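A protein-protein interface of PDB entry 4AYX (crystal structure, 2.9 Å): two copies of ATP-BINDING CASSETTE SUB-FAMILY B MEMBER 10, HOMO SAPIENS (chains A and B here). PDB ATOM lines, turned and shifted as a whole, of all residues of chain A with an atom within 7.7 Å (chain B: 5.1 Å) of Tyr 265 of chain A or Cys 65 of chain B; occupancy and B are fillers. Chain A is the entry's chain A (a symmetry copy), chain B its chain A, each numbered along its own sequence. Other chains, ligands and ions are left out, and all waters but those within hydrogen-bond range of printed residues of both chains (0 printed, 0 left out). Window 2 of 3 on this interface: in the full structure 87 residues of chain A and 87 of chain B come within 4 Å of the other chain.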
ATOM      1  N   LEU A 164     -19.286  27.240  -4.954  1.00  0.00           N
ATOM      2  CA  LEU A 164     -18.080  27.263  -4.124  1.00  0.00           C
ATOM      3  C   LEU A 164     -17.020  28.213  -4.681  1.00  0.00           C
ATOM      4  O   LEU A 164     -16.347  28.874  -3.891  1.00  0.00           O
ATOM      5  CB  LEU A 164     -17.471  25.865  -3.965  1.00  0.00           C
ATOM      6  CG  LEU A 164     -17.953  24.987  -2.822  1.00  0.00           C
ATOM      7  CD1 LEU A 164     -17.168  23.700  -2.802  1.00  0.00           C
ATOM      8  CD2 LEU A 164     -17.764  25.664  -1.481  1.00  0.00           C
ATOM      9  N   PHE A 167     -17.966  31.830  -3.951  1.00  0.00           N
ATOM     10  CA  PHE A 167     -17.773  32.004  -2.511  1.00  0.00           C
ATOM     11  C   PHE A 167     -16.294  32.347  -2.217  1.00  0.00           C
ATOM     12  O   PHE A 167     -16.021  33.350  -1.556  1.00  0.00           O
ATOM     13  CB  PHE A 167     -18.245  30.744  -1.741  1.00  0.00           C
ATOM     14  CG  PHE A 167     -17.889  30.751  -0.276  1.00  0.00           C
ATOM     15  CD1 PHE A 167     -18.593  31.543   0.623  1.00  0.00           C
ATOM     16  CD2 PHE A 167     -16.825  29.995   0.201  1.00  0.00           C
ATOM     17  CE1 PHE A 167     -18.232  31.587   1.970  1.00  0.00           C
ATOM     18  CE2 PHE A 167     -16.468  30.037   1.547  1.00  0.00           C
ATOM     19  CZ  PHE A 167     -17.174  30.832   2.422  1.00  0.00           C
ATOM     20  N   LEU A 258      -9.173  29.544   8.329  1.00  0.00           N
ATOM     21  CA  LEU A 258     -10.614  29.805   8.332  1.00  0.00           C
ATOM     22  C   LEU A 258     -11.194  29.876   6.914  1.00  0.00           C
ATOM     23  O   LEU A 258     -12.391  29.660   6.762  1.00  0.00           O
ATOM     24  CB  LEU A 258     -10.965  31.090   9.100  1.00  0.00           C
ATOM     25  CG  LEU A 258     -10.649  31.161  10.605  1.00  0.00           C
ATOM     26  CD1 LEU A 258     -11.022  32.507  11.149  1.00  0.00           C
ATOM     27  CD2 LEU A 258     -11.364  30.076  11.409  1.00  0.00           C
ATOM     28  N   ILE A 259     -10.372  30.171   5.886  1.00  0.00           N
ATOM     29  CA  ILE A 259     -10.844  30.197   4.495  1.00  0.00           C
ATOM     30  C   ILE A 259     -11.014  28.733   4.043  1.00  0.00           C
ATOM     31  O   ILE A 259     -12.081  28.375   3.534  1.00  0.00           O
ATOM     32  CB  ILE A 259      -9.939  31.050   3.545  1.00  0.00           C
ATOM     33  CG1 ILE A 259     -10.186  32.557   3.797  1.00  0.00           C
ATOM     34  CG2 ILE A 259     -10.201  30.715   2.068  1.00  0.00           C
ATOM     35  CD1 ILE A 259      -9.117  33.504   3.355  1.00  0.00           C
ATOM     36  N   VAL A 260      -9.982  27.888   4.296  1.00  0.00           N
ATOM     37  CA  VAL A 260      -9.970  26.445   4.009  1.00  0.00           C
ATOM     38  C   VAL A 260     -11.143  25.783   4.735  1.00  0.00           C
ATOM     39  O   VAL A 260     -11.869  24.997   4.115  1.00  0.00           O
ATOM     40  CB  VAL A 260      -8.617  25.794   4.413  1.00  0.00           C
ATOM     41  CG1 VAL A 260      -8.643  24.276   4.245  1.00  0.00           C
ATOM     42  CG2 VAL A 260      -7.455  26.408   3.638  1.00  0.00           C
ATOM     43  N   LEU A 261     -11.348  26.133   6.030  1.00  0.00           N
ATOM     44  CA  LEU A 261     -12.420  25.595   6.866  1.00  0.00           C
ATOM     45  C   LEU A 261     -13.792  25.945   6.292  1.00  0.00           C
ATOM     46  O   LEU A 261     -14.672  25.089   6.298  1.00  0.00           O
ATOM     47  CB  LEU A 261     -12.286  26.101   8.307  1.00  0.00           C
ATOM     48  CG  LEU A 261     -13.059  25.343   9.376  1.00  0.00           C
ATOM     49  CD1 LEU A 261     -12.483  23.954   9.597  1.00  0.00           C
ATOM     50  CD2 LEU A 261     -13.070  26.124  10.676  1.00  0.00           C
ATOM     51  N   SER A 262     -13.956  27.176   5.761  1.00  0.00           N
ATOM     52  CA  SER A 262     -15.194  27.656   5.143  1.00  0.00           C
ATOM     53  C   SER A 262     -15.550  26.838   3.914  1.00  0.00           C
ATOM     54  O   SER A 262     -16.722  26.558   3.687  1.00  0.00           O
ATOM     55  CB  SER A 262     -15.059  29.118   4.742  1.00  0.00           C
ATOM     56  OG  SER A 262     -15.013  29.963   5.877  1.00  0.00           O
ATOM     57  N   VAL A 263     -14.533  26.457   3.126  1.00  0.00           N
ATOM     58  CA  VAL A 263     -14.700  25.683   1.900  1.00  0.00           C
ATOM     59  C   VAL A 263     -15.036  24.228   2.273  1.00  0.00           C
ATOM     60  O   VAL A 263     -15.900  23.639   1.626  1.00  0.00           O
ATOM     61  CB  VAL A 263     -13.471  25.812   0.963  1.00  0.00           C
ATOM     62  CG1 VAL A 263     -13.666  25.018  -0.329  1.00  0.00           C
ATOM     63  CG2 VAL A 263     -13.188  27.281   0.647  1.00  0.00           C
ATOM     64  N   LEU A 264     -14.407  23.677   3.334  1.00  0.00           N
ATOM     65  CA  LEU A 264     -14.692  22.316   3.812  1.00  0.00           C
ATOM     66  C   LEU A 264     -16.117  22.233   4.371  1.00  0.00           C
ATOM     67  O   LEU A 264     -16.819  21.251   4.130  1.00  0.00           O
ATOM     68  CB  LEU A 264     -13.682  21.890   4.886  1.00  0.00           C
ATOM     69  CG  LEU A 264     -12.257  21.597   4.426  1.00  0.00           C
ATOM     70  CD1 LEU A 264     -11.319  21.588   5.607  1.00  0.00           C
ATOM     71  CD2 LEU A 264     -12.177  20.262   3.700  1.00  0.00           C
ATOM     72  N   TYR A 265     -16.545  23.286   5.089  1.00  0.00           N
ATOM     73  CA  TYR A 265     -17.871  23.398   5.670  1.00  0.00           C
ATOM     74  C   TYR A 265     -18.933  23.588   4.593  1.00  0.00           C
ATOM     75  O   TYR A 265     -19.860  22.795   4.545  1.00  0.00           O
ATOM     76  CB  TYR A 265     -17.925  24.539   6.681  1.00  0.00           C
ATOM     77  CG  TYR A 265     -19.283  24.722   7.321  1.00  0.00           C
ATOM     78  CD1 TYR A 265     -19.836  23.730   8.126  1.00  0.00           C
ATOM     79  CD2 TYR A 265     -19.994  25.910   7.166  1.00  0.00           C
ATOM     80  CE1 TYR A 265     -21.083  23.899   8.726  1.00  0.00           C
ATOM     81  CE2 TYR A 265     -21.236  26.092   7.768  1.00  0.00           C
ATOM     82  CZ  TYR A 265     -21.780  25.082   8.544  1.00  0.00           C
ATOM     83  OH  TYR A 265     -23.007  25.258   9.135  1.00  0.00           O
ATOM     84  N   LYS A 266     -18.799  24.617   3.730  1.00  0.00           N
ATOM     85  CA  LYS A 266     -19.758  24.906   2.651  1.00  0.00           C
ATOM     86  C   LYS A 266     -19.862  23.719   1.700  1.00  0.00           C
ATOM     87  O   LYS A 266     -20.982  23.325   1.346  1.00  0.00           O
ATOM     88  CB  LYS A 266     -19.381  26.182   1.892  1.00  0.00           C
ATOM     89  CG  LYS A 266     -20.506  26.751   1.054  1.00  0.00           C
ATOM     90  CD  LYS A 266     -20.438  28.256   1.035  1.00  0.00           C
ATOM     91  CE  LYS A 266     -21.252  28.849  -0.081  1.00  0.00           C
ATOM     92  NZ  LYS A 266     -22.695  28.583   0.099  1.00  0.00           N
ATOM     93  N   GLY A 267     -18.706  23.142   1.344  1.00  0.00           N
ATOM     94  CA  GLY A 267     -18.598  21.956   0.499  1.00  0.00           C
ATOM     95  C   GLY A 267     -19.256  20.752   1.146  1.00  0.00           C
ATOM     96  O   GLY A 267     -20.069  20.069   0.513  1.00  0.00           O
ATOM     97  N   GLY A 268     -18.950  20.542   2.431  1.00  0.00           N
ATOM     98  CA  GLY A 268     -19.523  19.467   3.237  1.00  0.00           C
ATOM     99  C   GLY A 268     -21.039  19.496   3.274  1.00  0.00           C
ATOM    100  O   GLY A 268     -21.677  18.447   3.155  1.00  0.00           O
ATOM    101  N   LEU A 269     -21.620  20.714   3.426  1.00  0.00           N
ATOM    102  CA  LEU A 269     -23.070  20.960   3.433  1.00  0.00           C
ATOM    103  C   LEU A 269     -23.669  20.657   2.065  1.00  0.00           C
ATOM    104  O   LEU A 269     -24.749  20.062   1.991  1.00  0.00           O
ATOM    105  CB  LEU A 269     -23.422  22.416   3.821  1.00  0.00           C
ATOM    106  CG  LEU A 269     -23.164  22.900   5.236  1.00  0.00           C
ATOM    107  CD1 LEU A 269     -23.476  24.366   5.339  1.00  0.00           C
ATOM    108  CD2 LEU A 269     -23.973  22.144   6.254  1.00  0.00           C
ATOM    109  N   LEU A 270     -22.964  21.080   0.978  1.00  0.00           N
ATOM    110  CA  LEU A 270     -23.390  20.864  -0.408  1.00  0.00           C
ATOM    111  C   LEU A 270     -23.374  19.373  -0.756  1.00  0.00           C
ATOM    112  O   LEU A 270     -24.197  18.932  -1.557  1.00  0.00           O
ATOM    113  CB  LEU A 270     -22.529  21.660  -1.396  1.00  0.00           C
ATOM    114  CG  LEU A 270     -22.766  23.170  -1.476  1.00  0.00           C
ATOM    115  CD1 LEU A 270     -21.618  23.852  -2.175  1.00  0.00           C
ATOM    116  CD2 LEU A 270     -24.049  23.490  -2.209  1.00  0.00           C
ATOM    117  N   MET A 271     -22.466  18.598  -0.131  1.00  0.00           N
ATOM    118  CA  MET A 271     -22.373  17.147  -0.296  1.00  0.00           C
ATOM    119  C   MET A 271     -23.641  16.489   0.233  1.00  0.00           C
ATOM    120  O   MET A 271     -24.300  15.767  -0.516  1.00  0.00           O
ATOM    121  CB  MET A 271     -21.157  16.580   0.443  1.00  0.00           C
ATOM    122  CG  MET A 271     -19.858  16.681  -0.287  1.00  0.00           C
ATOM    123  SD  MET A 271     -18.746  15.431   0.400  1.00  0.00           S
ATOM    124  CE  MET A 271     -18.075  16.279   1.668  1.00  0.00           C
ATOM    125  N   MET A 276     -23.050  17.976  -4.490  1.00  0.00           N
ATOM    126  CA  MET A 276     -21.666  17.543  -4.766  1.00  0.00           C
ATOM    127  C   MET A 276     -21.325  16.161  -4.207  1.00  0.00           C
ATOM    128  O   MET A 276     -21.980  15.698  -3.273  1.00  0.00           O
ATOM    129  CB  MET A 276     -20.666  18.523  -4.145  1.00  0.00           C
ATOM    130  CG  MET A 276     -20.545  19.836  -4.853  1.00  0.00           C
ATOM    131  SD  MET A 276     -19.080  20.696  -4.279  1.00  0.00           S
ATOM    132  CE  MET A 276     -19.282  20.564  -2.586  1.00  0.00           C
ATOM    133  N   LEU A 281     -15.494  17.416  -4.346  1.00  0.00           N
ATOM    134  CA  LEU A 281     -14.932  18.326  -3.356  1.00  0.00           C
ATOM    135  C   LEU A 281     -13.407  18.218  -3.363  1.00  0.00           C
ATOM    136  O   LEU A 281     -12.743  19.259  -3.412  1.00  0.00           O
ATOM    137  CB  LEU A 281     -15.494  18.095  -1.951  1.00  0.00           C
ATOM    138  CG  LEU A 281     -15.110  19.140  -0.875  1.00  0.00           C
ATOM    139  CD1 LEU A 281     -15.579  20.552  -1.243  1.00  0.00           C
ATOM    140  CD2 LEU A 281     -15.654  18.747   0.472  1.00  0.00           C
ATOM    141  N   ASN B  60     -22.951  17.442  13.144  1.00  0.00           N
ATOM    142  CA  ASN B  60     -21.595  16.978  13.449  1.00  0.00           C
ATOM    143  C   ASN B  60     -20.541  17.857  12.788  1.00  0.00           C
ATOM    144  O   ASN B  60     -19.553  18.203  13.435  1.00  0.00           O
ATOM    145  CB  ASN B  60     -21.411  15.527  13.017  1.00  0.00           C
ATOM    146  CG  ASN B  60     -22.315  14.574  13.749  1.00  0.00           C
ATOM    147  OD1 ASN B  60     -22.029  14.152  14.876  1.00  0.00           O
ATOM    148  ND2 ASN B  60     -23.441  14.245  13.135  1.00  0.00           N
ATOM    149  N   LEU B  61     -20.771  18.230  11.511  1.00  0.00           N
ATOM    150  CA  LEU B  61     -19.917  19.095  10.697  1.00  0.00           C
ATOM    151  C   LEU B  61     -19.864  20.497  11.312  1.00  0.00           C
ATOM    152  O   LEU B  61     -18.769  20.977  11.583  1.00  0.00           O
ATOM    153  CB  LEU B  61     -20.451  19.127   9.247  1.00  0.00           C
ATOM    154  CG  LEU B  61     -19.747  19.990   8.186  1.00  0.00           C
ATOM    155  CD1 LEU B  61     -18.304  19.534   7.930  1.00  0.00           C
ATOM    156  CD2 LEU B  61     -20.527  19.958   6.879  1.00  0.00           C
ATOM    157  N   THR B  62     -21.031  21.111  11.601  1.00  0.00           N
ATOM    158  CA  THR B  62     -21.152  22.441  12.214  1.00  0.00           C
ATOM    159  C   THR B  62     -20.464  22.477  13.604  1.00  0.00           C
ATOM    160  O   THR B  62     -19.750  23.440  13.900  1.00  0.00           O
ATOM    161  CB  THR B  62     -22.633  22.857  12.304  1.00  0.00           C
ATOM    162  OG1 THR B  62     -23.249  22.650  11.037  1.00  0.00           O
ATOM    163  CG2 THR B  62     -22.818  24.312  12.702  1.00  0.00           C
ATOM    164  N   ARG B  63     -20.664  21.431  14.435  1.00  0.00           N
ATOM    165  CA  ARG B  63     -20.052  21.335  15.765  1.00  0.00           C
ATOM    166  C   ARG B  63     -18.537  21.152  15.654  1.00  0.00           C
ATOM    167  O   ARG B  63     -17.811  21.721  16.469  1.00  0.00           O
ATOM    168  CB  ARG B  63     -20.676  20.192  16.586  1.00  0.00           C
ATOM    169  N   LEU B  64     -18.065  20.374  14.642  1.00  0.00           N
ATOM    170  CA  LEU B  64     -16.641  20.119  14.405  1.00  0.00           C
ATOM    171  C   LEU B  64     -15.952  21.365  13.862  1.00  0.00           C
ATOM    172  O   LEU B  64     -14.851  21.688  14.315  1.00  0.00           O
ATOM    173  CB  LEU B  64     -16.421  18.931  13.455  1.00  0.00           C
ATOM    174  CG  LEU B  64     -14.974  18.549  13.106  1.00  0.00           C
ATOM    175  CD1 LEU B  64     -14.237  17.950  14.303  1.00  0.00           C
ATOM    176  CD2 LEU B  64     -14.946  17.569  11.951  1.00  0.00           C
ATOM    177  N   CYS B  65     -16.598  22.067  12.912  1.00  0.00           N
ATOM    178  CA  CYS B  65     -16.057  23.289  12.319  1.00  0.00           C
ATOM    179  C   CYS B  65     -16.007  24.431  13.351  1.00  0.00           C
ATOM    180  O   CYS B  65     -15.026  25.172  13.358  1.00  0.00           O
ATOM    181  CB  CYS B  65     -16.834  23.686  11.072  1.00  0.00           C
ATOM    182  SG  CYS B  65     -16.609  22.552   9.675  1.00  0.00           S
ATOM    183  N   LEU B  66     -17.010  24.544  14.245  1.00  0.00           N
ATOM    184  CA  LEU B  66     -16.992  25.559  15.310  1.00  0.00           C
ATOM    185  C   LEU B  66     -15.901  25.230  16.326  1.00  0.00           C
ATOM    186  O   LEU B  66     -15.227  26.138  16.813  1.00  0.00           O
ATOM    187  CB  LEU B  66     -18.352  25.702  16.000  1.00  0.00           C
ATOM    188  CG  LEU B  66     -19.173  26.923  15.577  1.00  0.00           C
ATOM    189  CD1 LEU B  66     -19.813  26.730  14.194  1.00  0.00           C
ATOM    190  CD2 LEU B  66     -20.262  27.198  16.567  1.00  0.00           C
ATOM    191  N   GLY B  67     -15.691  23.939  16.574  1.00  0.00           N
ATOM    192  CA  GLY B  67     -14.638  23.447  17.452  1.00  0.00           C
ATOM    193  C   GLY B  67     -13.270  23.732  16.865  1.00  0.00           C
ATOM    194  O   GLY B  67     -12.403  24.264  17.565  1.00  0.00           O
ATOM    195  N   LEU B  68     -13.087  23.434  15.549  1.00  0.00           N
ATOM    196  CA  LEU B  68     -11.834  23.671  14.819  1.00  0.00           C
ATOM    197  C   LEU B  68     -11.504  25.158  14.728  1.00  0.00           C
ATOM    198  O   LEU B  68     -10.325  25.497  14.744  1.00  0.00           O
ATOM    199  CB  LEU B  68     -11.870  23.065  13.414  1.00  0.00           C
ATOM    200  CG  LEU B  68     -11.566  21.577  13.311  1.00  0.00           C
ATOM    201  CD1 LEU B  68     -12.036  21.039  12.000  1.00  0.00           C
ATOM    202  CD2 LEU B  68     -10.085  21.289  13.477  1.00  0.00           C
ATOM    203  N   SER B  69     -12.530  26.038  14.660  1.00  0.00           N
ATOM    204  CA  SER B  69     -12.385  27.500  14.637  1.00  0.00           C
ATOM    205  C   SER B  69     -11.682  27.985  15.904  1.00  0.00           C
ATOM    206  O   SER B  69     -10.718  28.737  15.806  1.00  0.00           O
ATOM    207  CB  SER B  69     -13.748  28.178  14.508  1.00  0.00           C
ATOM    208  OG  SER B  69     -14.256  28.080  13.189  1.00  0.00           O
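OG1 of Thr 62 of chain B is in hydrogen-bond range of OH of Tyr 265 of chain A, 3.2 Å away.
O of Leu 61 of chain B sits at hydrogen-bond distance from SG of Cys 65 of chain B, at 3.3 Å. The backbone carbonyl oxygen (O) of Cys 65 of chain B sits at hydrogen-bond distance from the side-chain hydroxyl (OG) of Ser 69 of chain B (3.0 Å). The backbone carbonyl oxygen (O) of Leu 258 of chain A lies within hydrogen-bond range of the side-chain hydroxyl (OG) of Ser 262 of chain A (2.8 Å).
No position is printed for both chains. Of the 9 pairs that touch across the chains among the printed residues, none has its exchanged pair printed and touching as well.
OG of Ser 69 of chain B touches CD2 of Leu 258 of chain A, 3.9 Å away. Cys 65 of chain B touches Leu 261 of chain A. Leu 261 of chain A touches Leu 68 of chain B (CD1 to CD1, 3.8 Å). Leu 261 of chain A touches Ser 69 of chain B. Tyr 265 of chain A touches Leu 61 of chain B. Tyr 265 of chain A touches Cys 65 of chain B (CD1 to SG, 3.8 Å). Leu 61 of chain B touches Gly 268 of chain A. Leu 269 of chain A touches Leu 61 of chain B (N to CD2, 3.7 Å).
Hydrophobic or aromatic side chains of chain A within 4 Å of the printed part of chain B: Leu 258, Leu 261 and Tyr 265. Of the 10 printed residues of chain B, 5 touch a printed residue of chain A. Hydrophobic or aromatic side chains of chain B that line the printed part of chain A: Leu 61 and Leu 68.
Tyr 265 of chain A touches just these residues of chain B: Leu 61 (3.7 Å), Thr 62 (3.2 Å) and Cys 65 (3.8 Å). Cys 65 of chain B touches two residues of chain A. Of the printed residues of chain A, Thr 62 of chain B touches Tyr 265 (3.2 Å). Of the printed residues of chain B, Leu 261 of chain A touches Cys 65 (3.5 Å), Leu 68 (3.8 Å) and Ser 69 (3.4 Å). Printed residues of chain B within 4 Å of Leu 269 of chain A: Leu 61 (3.7 Å). Printed residues of chain B within 4 Å of Gly 268 of chain A: Leu 61 (3.7 Å). Of the printed residues of chain A, Ser 69 of chain B touches Leu 258 (3.9 Å) and Leu 261 (3.4 Å). Leu 164 of chain A touches none of the printed residues of chain B. Leu 270 of chain A touches none of the printed residues of chain B.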
